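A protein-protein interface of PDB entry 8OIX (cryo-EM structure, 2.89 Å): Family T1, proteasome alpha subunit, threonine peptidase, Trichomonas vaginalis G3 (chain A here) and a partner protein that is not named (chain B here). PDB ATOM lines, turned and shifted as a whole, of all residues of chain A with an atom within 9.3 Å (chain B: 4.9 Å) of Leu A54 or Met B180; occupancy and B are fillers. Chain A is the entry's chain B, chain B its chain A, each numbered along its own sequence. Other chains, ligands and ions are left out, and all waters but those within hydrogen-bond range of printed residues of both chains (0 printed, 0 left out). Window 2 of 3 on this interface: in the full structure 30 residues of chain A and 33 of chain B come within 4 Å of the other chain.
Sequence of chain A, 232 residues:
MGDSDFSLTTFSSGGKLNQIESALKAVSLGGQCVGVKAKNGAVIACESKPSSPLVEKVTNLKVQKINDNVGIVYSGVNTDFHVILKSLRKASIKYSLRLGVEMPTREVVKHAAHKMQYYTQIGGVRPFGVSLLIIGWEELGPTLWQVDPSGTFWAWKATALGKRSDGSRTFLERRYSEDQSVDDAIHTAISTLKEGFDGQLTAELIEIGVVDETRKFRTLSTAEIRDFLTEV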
ATOM      1  N   PRO A  50     -10.177  10.884  28.200  1.00  0.00           N
ATOM      2  CA  PRO A  50     -11.104   9.753  28.180  1.00  0.00           C
ATOM      3  C   PRO A  50     -10.379   8.430  28.352  1.00  0.00           C
ATOM      4  O   PRO A  50      -9.158   8.329  28.200  1.00  0.00           O
ATOM      5  CB  PRO A  50     -11.756   9.854  26.797  1.00  0.00           C
ATOM      6  CG  PRO A  50     -10.769  10.587  25.967  1.00  0.00           C
ATOM      7  CD  PRO A  50     -10.080  11.548  26.889  1.00  0.00           C
ATOM      8  N   SER A  51     -11.161   7.406  28.703  1.00  0.00           N
ATOM      9  CA  SER A  51     -10.628   6.050  28.776  1.00  0.00           C
ATOM     10  C   SER A  51      -9.918   5.674  27.484  1.00  0.00           C
ATOM     11  O   SER A  51      -8.862   5.031  27.505  1.00  0.00           O
ATOM     12  CB  SER A  51     -11.755   5.060  29.073  1.00  0.00           C
ATOM     13  OG  SER A  51     -12.611   5.551  30.087  1.00  0.00           O
ATOM     14  N   SER A  52     -10.483   6.071  26.349  1.00  0.00           N
ATOM     15  CA  SER A  52      -9.904   5.798  25.044  1.00  0.00           C
ATOM     16  C   SER A  52     -10.416   6.851  24.072  1.00  0.00           C
ATOM     17  O   SER A  52     -11.406   7.533  24.361  1.00  0.00           O
ATOM     18  CB  SER A  52     -10.277   4.390  24.557  1.00  0.00           C
ATOM     19  OG  SER A  52     -11.684   4.251  24.478  1.00  0.00           O
ATOM     20  N   PRO A  53      -9.759   7.017  22.921  1.00  0.00           N
ATOM     21  CA  PRO A  53     -10.292   7.941  21.906  1.00  0.00           C
ATOM     22  C   PRO A  53     -11.695   7.586  21.451  1.00  0.00           C
ATOM     23  O   PRO A  53     -12.364   8.423  20.832  1.00  0.00           O
ATOM     24  CB  PRO A  53      -9.282   7.822  20.758  1.00  0.00           C
ATOM     25  CG  PRO A  53      -8.016   7.409  21.422  1.00  0.00           C
ATOM     26  CD  PRO A  53      -8.420   6.518  22.561  1.00  0.00           C
ATOM     27  N   LEU A  54     -12.155   6.370  21.736  1.00  0.00           N
ATOM     28  CA  LEU A  54     -13.491   5.922  21.374  1.00  0.00           C
ATOM     29  C   LEU A  54     -14.570   6.449  22.309  1.00  0.00           C
ATOM     30  O   LEU A  54     -15.756   6.332  21.987  1.00  0.00           O
ATOM     31  CB  LEU A  54     -13.528   4.395  21.367  1.00  0.00           C
ATOM     32  CG  LEU A  54     -12.513   3.704  20.461  1.00  0.00           C
ATOM     33  CD1 LEU A  54     -12.389   2.244  20.839  1.00  0.00           C
ATOM     34  CD2 LEU A  54     -12.923   3.847  19.008  1.00  0.00           C
ATOM     35  N   VAL A  55     -14.191   7.019  23.454  1.00  0.00           N
ATOM     36  CA  VAL A  55     -15.171   7.566  24.383  1.00  0.00           C
ATOM     37  C   VAL A  55     -15.772   8.836  23.799  1.00  0.00           C
ATOM     38  O   VAL A  55     -15.073   9.651  23.182  1.00  0.00           O
ATOM     39  CB  VAL A  55     -14.513   7.845  25.746  1.00  0.00           C
ATOM     40  CG1 VAL A  55     -15.490   8.524  26.696  1.00  0.00           C
ATOM     41  CG2 VAL A  55     -13.964   6.570  26.352  1.00  0.00           C
ATOM     42  N   GLU A  56     -17.076   9.013  23.992  1.00  0.00           N
ATOM     43  CA  GLU A  56     -17.751  10.244  23.606  1.00  0.00           C
ATOM     44  C   GLU A  56     -17.746  11.195  24.795  1.00  0.00           C
ATOM     45  O   GLU A  56     -18.343  10.899  25.836  1.00  0.00           O
ATOM     46  CB  GLU A  56     -19.174   9.962  23.133  1.00  0.00           C
ATOM     47  CG  GLU A  56     -19.235   9.198  21.824  1.00  0.00           C
ATOM     48  CD  GLU A  56     -20.648   8.848  21.422  1.00  0.00           C
ATOM     49  OE1 GLU A  56     -21.579   9.127  22.208  1.00  0.00           O
ATOM     50  OE2 GLU A  56     -20.831   8.299  20.315  1.00  0.00           O
ATOM     51  N   LYS A  57     -17.066  12.332  24.635  1.00  0.00           N
ATOM     52  CA  LYS A  57     -16.812  13.229  25.759  1.00  0.00           C
ATOM     53  C   LYS A  57     -18.109  13.738  26.375  1.00  0.00           C
ATOM     54  O   LYS A  57     -18.272  13.720  27.604  1.00  0.00           O
ATOM     55  CB  LYS A  57     -15.943  14.394  25.284  1.00  0.00           C
ATOM     56  CG  LYS A  57     -15.454  15.329  26.370  1.00  0.00           C
ATOM     57  CD  LYS A  57     -14.956  16.624  25.748  1.00  0.00           C
ATOM     58  CE  LYS A  57     -14.483  17.605  26.800  1.00  0.00           C
ATOM     59  NZ  LYS A  57     -14.063  18.902  26.201  1.00  0.00           N
ATOM     60  N   VAL A  58     -19.066  14.139  25.532  1.00  0.00           N
ATOM     61  CA  VAL A  58     -20.279  14.795  26.014  1.00  0.00           C
ATOM     62  C   VAL A  58     -21.034  13.894  26.980  1.00  0.00           C
ATOM     63  O   VAL A  58     -21.759  14.377  27.859  1.00  0.00           O
ATOM     64  CB  VAL A  58     -21.159  15.221  24.821  1.00  0.00           C
ATOM     65  CG1 VAL A  58     -21.655  14.004  24.053  1.00  0.00           C
ATOM     66  CG2 VAL A  58     -22.322  16.087  25.285  1.00  0.00           C
ATOM     67  N   THR A  59     -20.866  12.581  26.852  1.00  0.00           N
ATOM     68  CA  THR A  59     -21.636  11.646  27.655  1.00  0.00           C
ATOM     69  C   THR A  59     -21.147  11.568  29.095  1.00  0.00           C
ATOM     70  O   THR A  59     -21.892  11.090  29.958  1.00  0.00           O
ATOM     71  CB  THR A  59     -21.588  10.253  27.028  1.00  0.00           C
ATOM     72  OG1 THR A  59     -20.234   9.788  27.000  1.00  0.00           O
ATOM     73  CG2 THR A  59     -22.124  10.297  25.607  1.00  0.00           C
ATOM     74  N   VAL B  38     -19.590  -1.768  18.116  1.00  0.00           N
ATOM     75  CA  VAL B  38     -19.171  -0.690  17.231  1.00  0.00           C
ATOM     76  C   VAL B  38     -20.404   0.117  16.860  1.00  0.00           C
ATOM     77  O   VAL B  38     -21.439  -0.452  16.494  1.00  0.00           O
ATOM     78  CB  VAL B  38     -18.462  -1.224  15.974  1.00  0.00           C
ATOM     79  CG1 VAL B  38     -17.985  -0.073  15.107  1.00  0.00           C
ATOM     80  CG2 VAL B  38     -17.298  -2.116  16.366  1.00  0.00           C
ATOM     81  N   LYS B  39     -20.293   1.438  16.946  1.00  0.00           N
ATOM     82  CA  LYS B  39     -21.386   2.337  16.609  1.00  0.00           C
ATOM     83  C   LYS B  39     -21.026   3.128  15.362  1.00  0.00           C
ATOM     84  O   LYS B  39     -19.920   3.667  15.257  1.00  0.00           O
ATOM     85  CB  LYS B  39     -21.695   3.289  17.764  1.00  0.00           C
ATOM     86  CG  LYS B  39     -23.013   4.014  17.610  1.00  0.00           C
ATOM     87  CD  LYS B  39     -22.864   5.486  17.926  1.00  0.00           C
ATOM     88  CE  LYS B  39     -22.574   5.709  19.393  1.00  0.00           C
ATOM     89  NZ  LYS B  39     -22.768   7.134  19.771  1.00  0.00           N
ATOM     90  N   GLY B 159     -20.248   7.195  26.838  1.00  0.00           N
ATOM     91  CA  GLY B 159     -20.712   6.930  25.491  1.00  0.00           C
ATOM     92  C   GLY B 159     -19.524   6.595  24.605  1.00  0.00           C
ATOM     93  O   GLY B 159     -18.469   7.217  24.696  1.00  0.00           O
ATOM     94  N   PHE B 160     -19.707   5.595  23.753  1.00  0.00           N
ATOM     95  CA  PHE B 160     -18.614   5.073  22.950  1.00  0.00           C
ATOM     96  C   PHE B 160     -18.984   5.042  21.478  1.00  0.00           C
ATOM     97  O   PHE B 160     -20.097   4.650  21.115  1.00  0.00           O
ATOM     98  CB  PHE B 160     -18.234   3.662  23.398  1.00  0.00           C
ATOM     99  CG  PHE B 160     -17.455   3.616  24.676  1.00  0.00           C
ATOM    100  CD1 PHE B 160     -18.101   3.576  25.896  1.00  0.00           C
ATOM    101  CD2 PHE B 160     -16.073   3.581  24.655  1.00  0.00           C
ATOM    102  CE1 PHE B 160     -17.384   3.523  27.069  1.00  0.00           C
ATOM    103  CE2 PHE B 160     -15.353   3.523  25.825  1.00  0.00           C
ATOM    104  CZ  PHE B 160     -16.008   3.497  27.034  1.00  0.00           C
ATOM    105  N   ARG B 161     -18.040   5.459  20.634  1.00  0.00           N
ATOM    106  CA  ARG B 161     -18.125   5.125  19.218  1.00  0.00           C
ATOM    107  C   ARG B 161     -17.908   3.632  19.017  1.00  0.00           C
ATOM    108  O   ARG B 161     -18.579   3.000  18.195  1.00  0.00           O
ATOM    109  CB  ARG B 161     -17.107   5.938  18.421  1.00  0.00           C
ATOM    110  CG  ARG B 161     -17.243   7.442  18.593  1.00  0.00           C
ATOM    111  CD  ARG B 161     -16.434   8.190  17.548  1.00  0.00           C
ATOM    112  NE  ARG B 161     -15.095   7.633  17.400  1.00  0.00           N
ATOM    113  CZ  ARG B 161     -14.051   7.977  18.142  1.00  0.00           C
ATOM    114  NH1 ARG B 161     -14.152   8.889  19.094  1.00  0.00           N
ATOM    115  NH2 ARG B 161     -12.878   7.393  17.922  1.00  0.00           N
ATOM    116  N   ALA B 162     -16.967   3.058  19.763  1.00  0.00           N
ATOM    117  CA  ALA B 162     -16.785   1.620  19.847  1.00  0.00           C
ATOM    118  C   ALA B 162     -16.291   1.297  21.247  1.00  0.00           C
ATOM    119  O   ALA B 162     -15.473   2.031  21.807  1.00  0.00           O
ATOM    120  CB  ALA B 162     -15.796   1.106  18.796  1.00  0.00           C
ATOM    121  N   MET B 173     -10.356  -3.056  22.920  1.00  0.00           N
ATOM    122  CA  MET B 173     -10.439  -1.601  22.830  1.00  0.00           C
ATOM    123  C   MET B 173      -9.273  -1.036  22.031  1.00  0.00           C
ATOM    124  O   MET B 173      -9.451  -0.098  21.242  1.00  0.00           O
ATOM    125  CB  MET B 173     -10.479  -0.984  24.227  1.00  0.00           C
ATOM    126  CG  MET B 173     -11.769  -1.241  24.982  1.00  0.00           C
ATOM    127  SD  MET B 173     -13.181  -0.405  24.253  1.00  0.00           S
ATOM    128  CE  MET B 173     -12.775   1.301  24.591  1.00  0.00           C
ATOM    129  N   ALA B 175      -7.600  -2.567  19.596  1.00  0.00           N
ATOM    130  CA  ALA B 175      -7.855  -2.859  18.189  1.00  0.00           C
ATOM    131  C   ALA B 175      -8.949  -1.958  17.629  1.00  0.00           C
ATOM    132  O   ALA B 175      -8.844  -1.469  16.497  1.00  0.00           O
ATOM    133  CB  ALA B 175      -8.229  -4.330  18.017  1.00  0.00           C
ATOM    134  N   LEU B 176      -9.999  -1.715  18.416  1.00  0.00           N
ATOM    135  CA  LEU B 176     -11.087  -0.854  17.969  1.00  0.00           C
ATOM    136  C   LEU B 176     -10.583   0.550  17.678  1.00  0.00           C
ATOM    137  O   LEU B 176     -10.832   1.099  16.599  1.00  0.00           O
ATOM    138  CB  LEU B 176     -12.195  -0.820  19.020  1.00  0.00           C
ATOM    139  CG  LEU B 176     -13.107  -2.040  19.132  1.00  0.00           C
ATOM    140  CD1 LEU B 176     -14.019  -1.902  20.335  1.00  0.00           C
ATOM    141  CD2 LEU B 176     -13.917  -2.215  17.866  1.00  0.00           C
ATOM    142  N   GLU B 177      -9.862   1.149  18.629  1.00  0.00           N
ATOM    143  CA  GLU B 177      -9.390   2.516  18.427  1.00  0.00           C
ATOM    144  C   GLU B 177      -8.368   2.587  17.298  1.00  0.00           C
ATOM    145  O   GLU B 177      -8.360   3.551  16.523  1.00  0.00           O
ATOM    146  CB  GLU B 177      -8.821   3.083  19.730  1.00  0.00           C
ATOM    147  CG  GLU B 177      -7.595   2.371  20.266  1.00  0.00           C
ATOM    148  CD  GLU B 177      -7.253   2.792  21.682  1.00  0.00           C
ATOM    149  OE1 GLU B 177      -8.188   3.075  22.459  1.00  0.00           O
ATOM    150  OE2 GLU B 177      -6.050   2.839  22.015  1.00  0.00           O
ATOM    151  N   LYS B 178      -7.499   1.579  17.181  1.00  0.00           N
ATOM    152  CA  LYS B 178      -6.532   1.543  16.091  1.00  0.00           C
ATOM    153  C   LYS B 178      -7.165   1.230  14.741  1.00  0.00           C
ATOM    154  O   LYS B 178      -6.487   1.368  13.718  1.00  0.00           O
ATOM    155  CB  LYS B 178      -5.437   0.521  16.398  1.00  0.00           C
ATOM    156  CG  LYS B 178      -4.503   0.941  17.522  1.00  0.00           C
ATOM    157  CD  LYS B 178      -3.351  -0.034  17.686  1.00  0.00           C
ATOM    158  CE  LYS B 178      -2.412   0.411  18.796  1.00  0.00           C
ATOM    159  NZ  LYS B 178      -1.368  -0.608  19.090  1.00  0.00           N
ATOM    160  N   LYS B 179      -8.435   0.812  14.705  1.00  0.00           N
ATOM    161  CA  LYS B 179      -9.080   0.509  13.434  1.00  0.00           C
ATOM    162  C   LYS B 179     -10.486   1.090  13.316  1.00  0.00           C
ATOM    163  O   LYS B 179     -11.220   0.701  12.398  1.00  0.00           O
ATOM    164  CB  LYS B 179      -9.140  -1.008  13.201  1.00  0.00           C
ATOM    165  CG  LYS B 179      -7.820  -1.741  13.386  1.00  0.00           C
ATOM    166  CD  LYS B 179      -7.928  -3.190  12.941  1.00  0.00           C
ATOM    167  CE  LYS B 179      -8.153  -3.289  11.440  1.00  0.00           C
ATOM    168  NZ  LYS B 179      -7.927  -4.668  10.928  1.00  0.00           N
ATOM    169  N   MET B 180     -10.888   1.994  14.205  1.00  0.00           N
ATOM    170  CA  MET B 180     -12.221   2.579  14.127  1.00  0.00           C
ATOM    171  C   MET B 180     -12.357   3.451  12.885  1.00  0.00           C
ATOM    172  O   MET B 180     -11.415   4.136  12.478  1.00  0.00           O
ATOM    173  CB  MET B 180     -12.515   3.404  15.378  1.00  0.00           C
ATOM    174  CG  MET B 180     -13.944   3.905  15.471  1.00  0.00           C
ATOM    175  SD  MET B 180     -15.138   2.557  15.490  1.00  0.00           S
ATOM    176  CE  MET B 180     -16.669   3.474  15.583  1.00  0.00           C
ATOM    177  N   GLU B 181     -13.546   3.424  12.282  1.00  0.00           N
ATOM    178  CA  GLU B 181     -13.838   4.198  11.086  1.00  0.00           C
ATOM    179  C   GLU B 181     -15.271   4.705  11.156  1.00  0.00           C
ATOM    180  O   GLU B 181     -16.108   4.162  11.881  1.00  0.00           O
ATOM    181  CB  GLU B 181     -13.652   3.372   9.802  1.00  0.00           C
ATOM    182  CG  GLU B 181     -12.361   2.573   9.724  1.00  0.00           C
ATOM    183  CD  GLU B 181     -12.278   1.722   8.473  1.00  0.00           C
ATOM    184  OE1 GLU B 181     -12.967   2.049   7.484  1.00  0.00           O
ATOM    185  OE2 GLU B 181     -11.526   0.726   8.480  1.00  0.00           O
ATOM    186  N   ASP B 182     -15.542   5.769  10.399  1.00  0.00           N
ATOM    187  CA  ASP B 182     -16.909   6.259  10.211  1.00  0.00           C
ATOM    188  C   ASP B 182     -17.543   5.468   9.071  1.00  0.00           C
ATOM    189  O   ASP B 182     -17.667   5.931   7.934  1.00  0.00           O
ATOM    190  CB  ASP B 182     -16.915   7.757   9.937  1.00  0.00           C
ATOM    191  CG  ASP B 182     -16.677   8.579  11.187  1.00  0.00           C
ATOM    192  OD1 ASP B 182     -16.379   7.984  12.244  1.00  0.00           O
ATOM    193  OD2 ASP B 182     -16.792   9.819  11.113  1.00  0.00           O
ATOM    194  N   PHE B 183     -17.935   4.236   9.391  1.00  0.00           N
ATOM    195  CA  PHE B 183     -18.477   3.322   8.395  1.00  0.00           C
ATOM    196  C   PHE B 183     -19.714   3.910   7.725  1.00  0.00           C
ATOM    197  O   PHE B 183     -20.473   4.675   8.326  1.00  0.00           O
ATOM    198  CB  PHE B 183     -18.805   1.979   9.042  1.00  0.00           C
ATOM    199  CG  PHE B 183     -17.631   1.350   9.722  1.00  0.00           C
ATOM    200  CD1 PHE B 183     -16.708   0.614   9.000  1.00  0.00           C
ATOM    201  CD2 PHE B 183     -17.437   1.507  11.082  1.00  0.00           C
ATOM    202  CE1 PHE B 183     -15.619   0.045   9.621  1.00  0.00           C
ATOM    203  CE2 PHE B 183     -16.350   0.938  11.709  1.00  0.00           C
ATOM    204  CZ  PHE B 183     -15.439   0.211  10.975  1.00  0.00           C
ATOM    205  N   PHE B 192     -16.785  -5.028  10.953  1.00  0.00           N
ATOM    206  CA  PHE B 192     -15.728  -4.558  11.842  1.00  0.00           C
ATOM    207  C   PHE B 192     -15.913  -5.098  13.252  1.00  0.00           C
ATOM    208  O   PHE B 192     -14.940  -5.495  13.902  1.00  0.00           O
ATOM    209  CB  PHE B 192     -15.686  -3.035  11.859  1.00  0.00           C
ATOM    210  CG  PHE B 192     -14.637  -2.475  12.773  1.00  0.00           C
ATOM    211  CD1 PHE B 192     -13.312  -2.846  12.631  1.00  0.00           C
ATOM    212  CD2 PHE B 192     -14.973  -1.575  13.767  1.00  0.00           C
ATOM    213  CE1 PHE B 192     -12.344  -2.333  13.467  1.00  0.00           C
ATOM    214  CE2 PHE B 192     -14.009  -1.056  14.602  1.00  0.00           C
ATOM    215  CZ  PHE B 192     -12.692  -1.437  14.454  1.00  0.00           C
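OE1 of Glu A56 is in salt-bridge range of NZ of Lys B39. The side-chain hydroxyl (OG1) of Thr A59 lies within hydrogen-bond range of the backbone NH (N) of Gly B159 (2.6 Å). The guanidinium group (NH1) of Arg B161 sits at hydrogen-bond distance from the backbone carbonyl oxygen (O) of Pro A53, 2.5 Å away. The backbone NH (N) of Arg B161 lies within hydrogen-bond range of the backbone carbonyl oxygen (O) of Leu A54, 2.8 Å away. O of Gly B159 lies close to N of Glu A56, at 2.4 Å.
N of Lys B39 lies within hydrogen-bond range of O of Arg B161 (2.6 Å). The side-chain hydroxyl (OG) of Ser A52 lies close to the backbone NH (N) of Leu A54 (3.5 Å). The side-chain hydroxyl of Thr A59 sits at hydrogen-bond distance from the backbone carbonyl oxygen of Glu A56 (2.5 Å).
Ser A52 touches Phe B160. Glu B177 touches Pro A53. Leu A54 touches Gly B159. CA of Phe B160 touches O of Leu A54, 3.3 Å away. CB of Leu A54 touches O of Ala B162, at 3.1 Å. O of Met B173 touches CD1 of Leu A54, at 3.8 Å. Leu A54 touches Glu B177. Leu A54 touches Met B180 (CD2 to CB, 3.7 Å). C of Val A55 touches O of Gly B159, at 3.3 Å. Val A55 touches Phe B160.
Leu A54 touches just these residues of chain B: Gly B159 (3.9 Å), Phe B160 (3.3 Å), Arg B161 (2.8 Å), Ala B162 (3.1 Å), Met B173 (3.8 Å), Leu B176 (3.6 Å), Glu B177 (3.5 Å) and Met B180 (3.7 Å). Met B180 touches just one residue of chain A: Leu A54 (3.7 Å). Of chain A, only Leu A54 (3.1 Å) comes within 4 Å of Ala B162. Of the printed residues of chain A, Leu B176 touches Leu A54 (3.6 Å). Of the printed residues of chain B, Val A55 touches Gly B159 (3.3 Å) and Phe B160 (3.4 Å). Printed residues of chain A within 4 Å of Arg B161: Pro A53 (2.5 Å), Leu A54 (2.8 Å) and Glu A56 (3.99 Å). Printed residues of chain B within 4 Å of Pro A53: Arg B161 (2.5 Å) and Glu B177 (3.5 Å). Of the printed residues of chain A, Lys B39 touches Glu A56 (2.3 Å). The nearest residue of chain A that does not touch Met B180 is Pro A53 (7.2 Å). The nearest printed residue of chain B that does not touch Pro A53 is Met B173 (6.7 Å).
Of the 17 printed residues of chain B, 9 touch a printed residue of chain A. Printed residues of chain B that touch a printed residue of chain A: Lys B39, Gly B159, Phe B160, Arg B161, Ala B162, Met B173, Leu B176, Glu B177 and Met B180. Along chain B the printed residues that touch a printed residue of chain A span positions 39 to 180. Of the 10 printed residues of chain A, 6 touch a printed residue of chain B. Hydrophobic or aromatic side chains of chain A within 4 Å of the printed part of chain B: Pro A53, Leu A54 and Val A55. Among the printed residues, Asp or Glu carboxylates within 4 Å of a Lys or Arg side-chain nitrogen of the other chain: Glu A56 with Lys B39.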
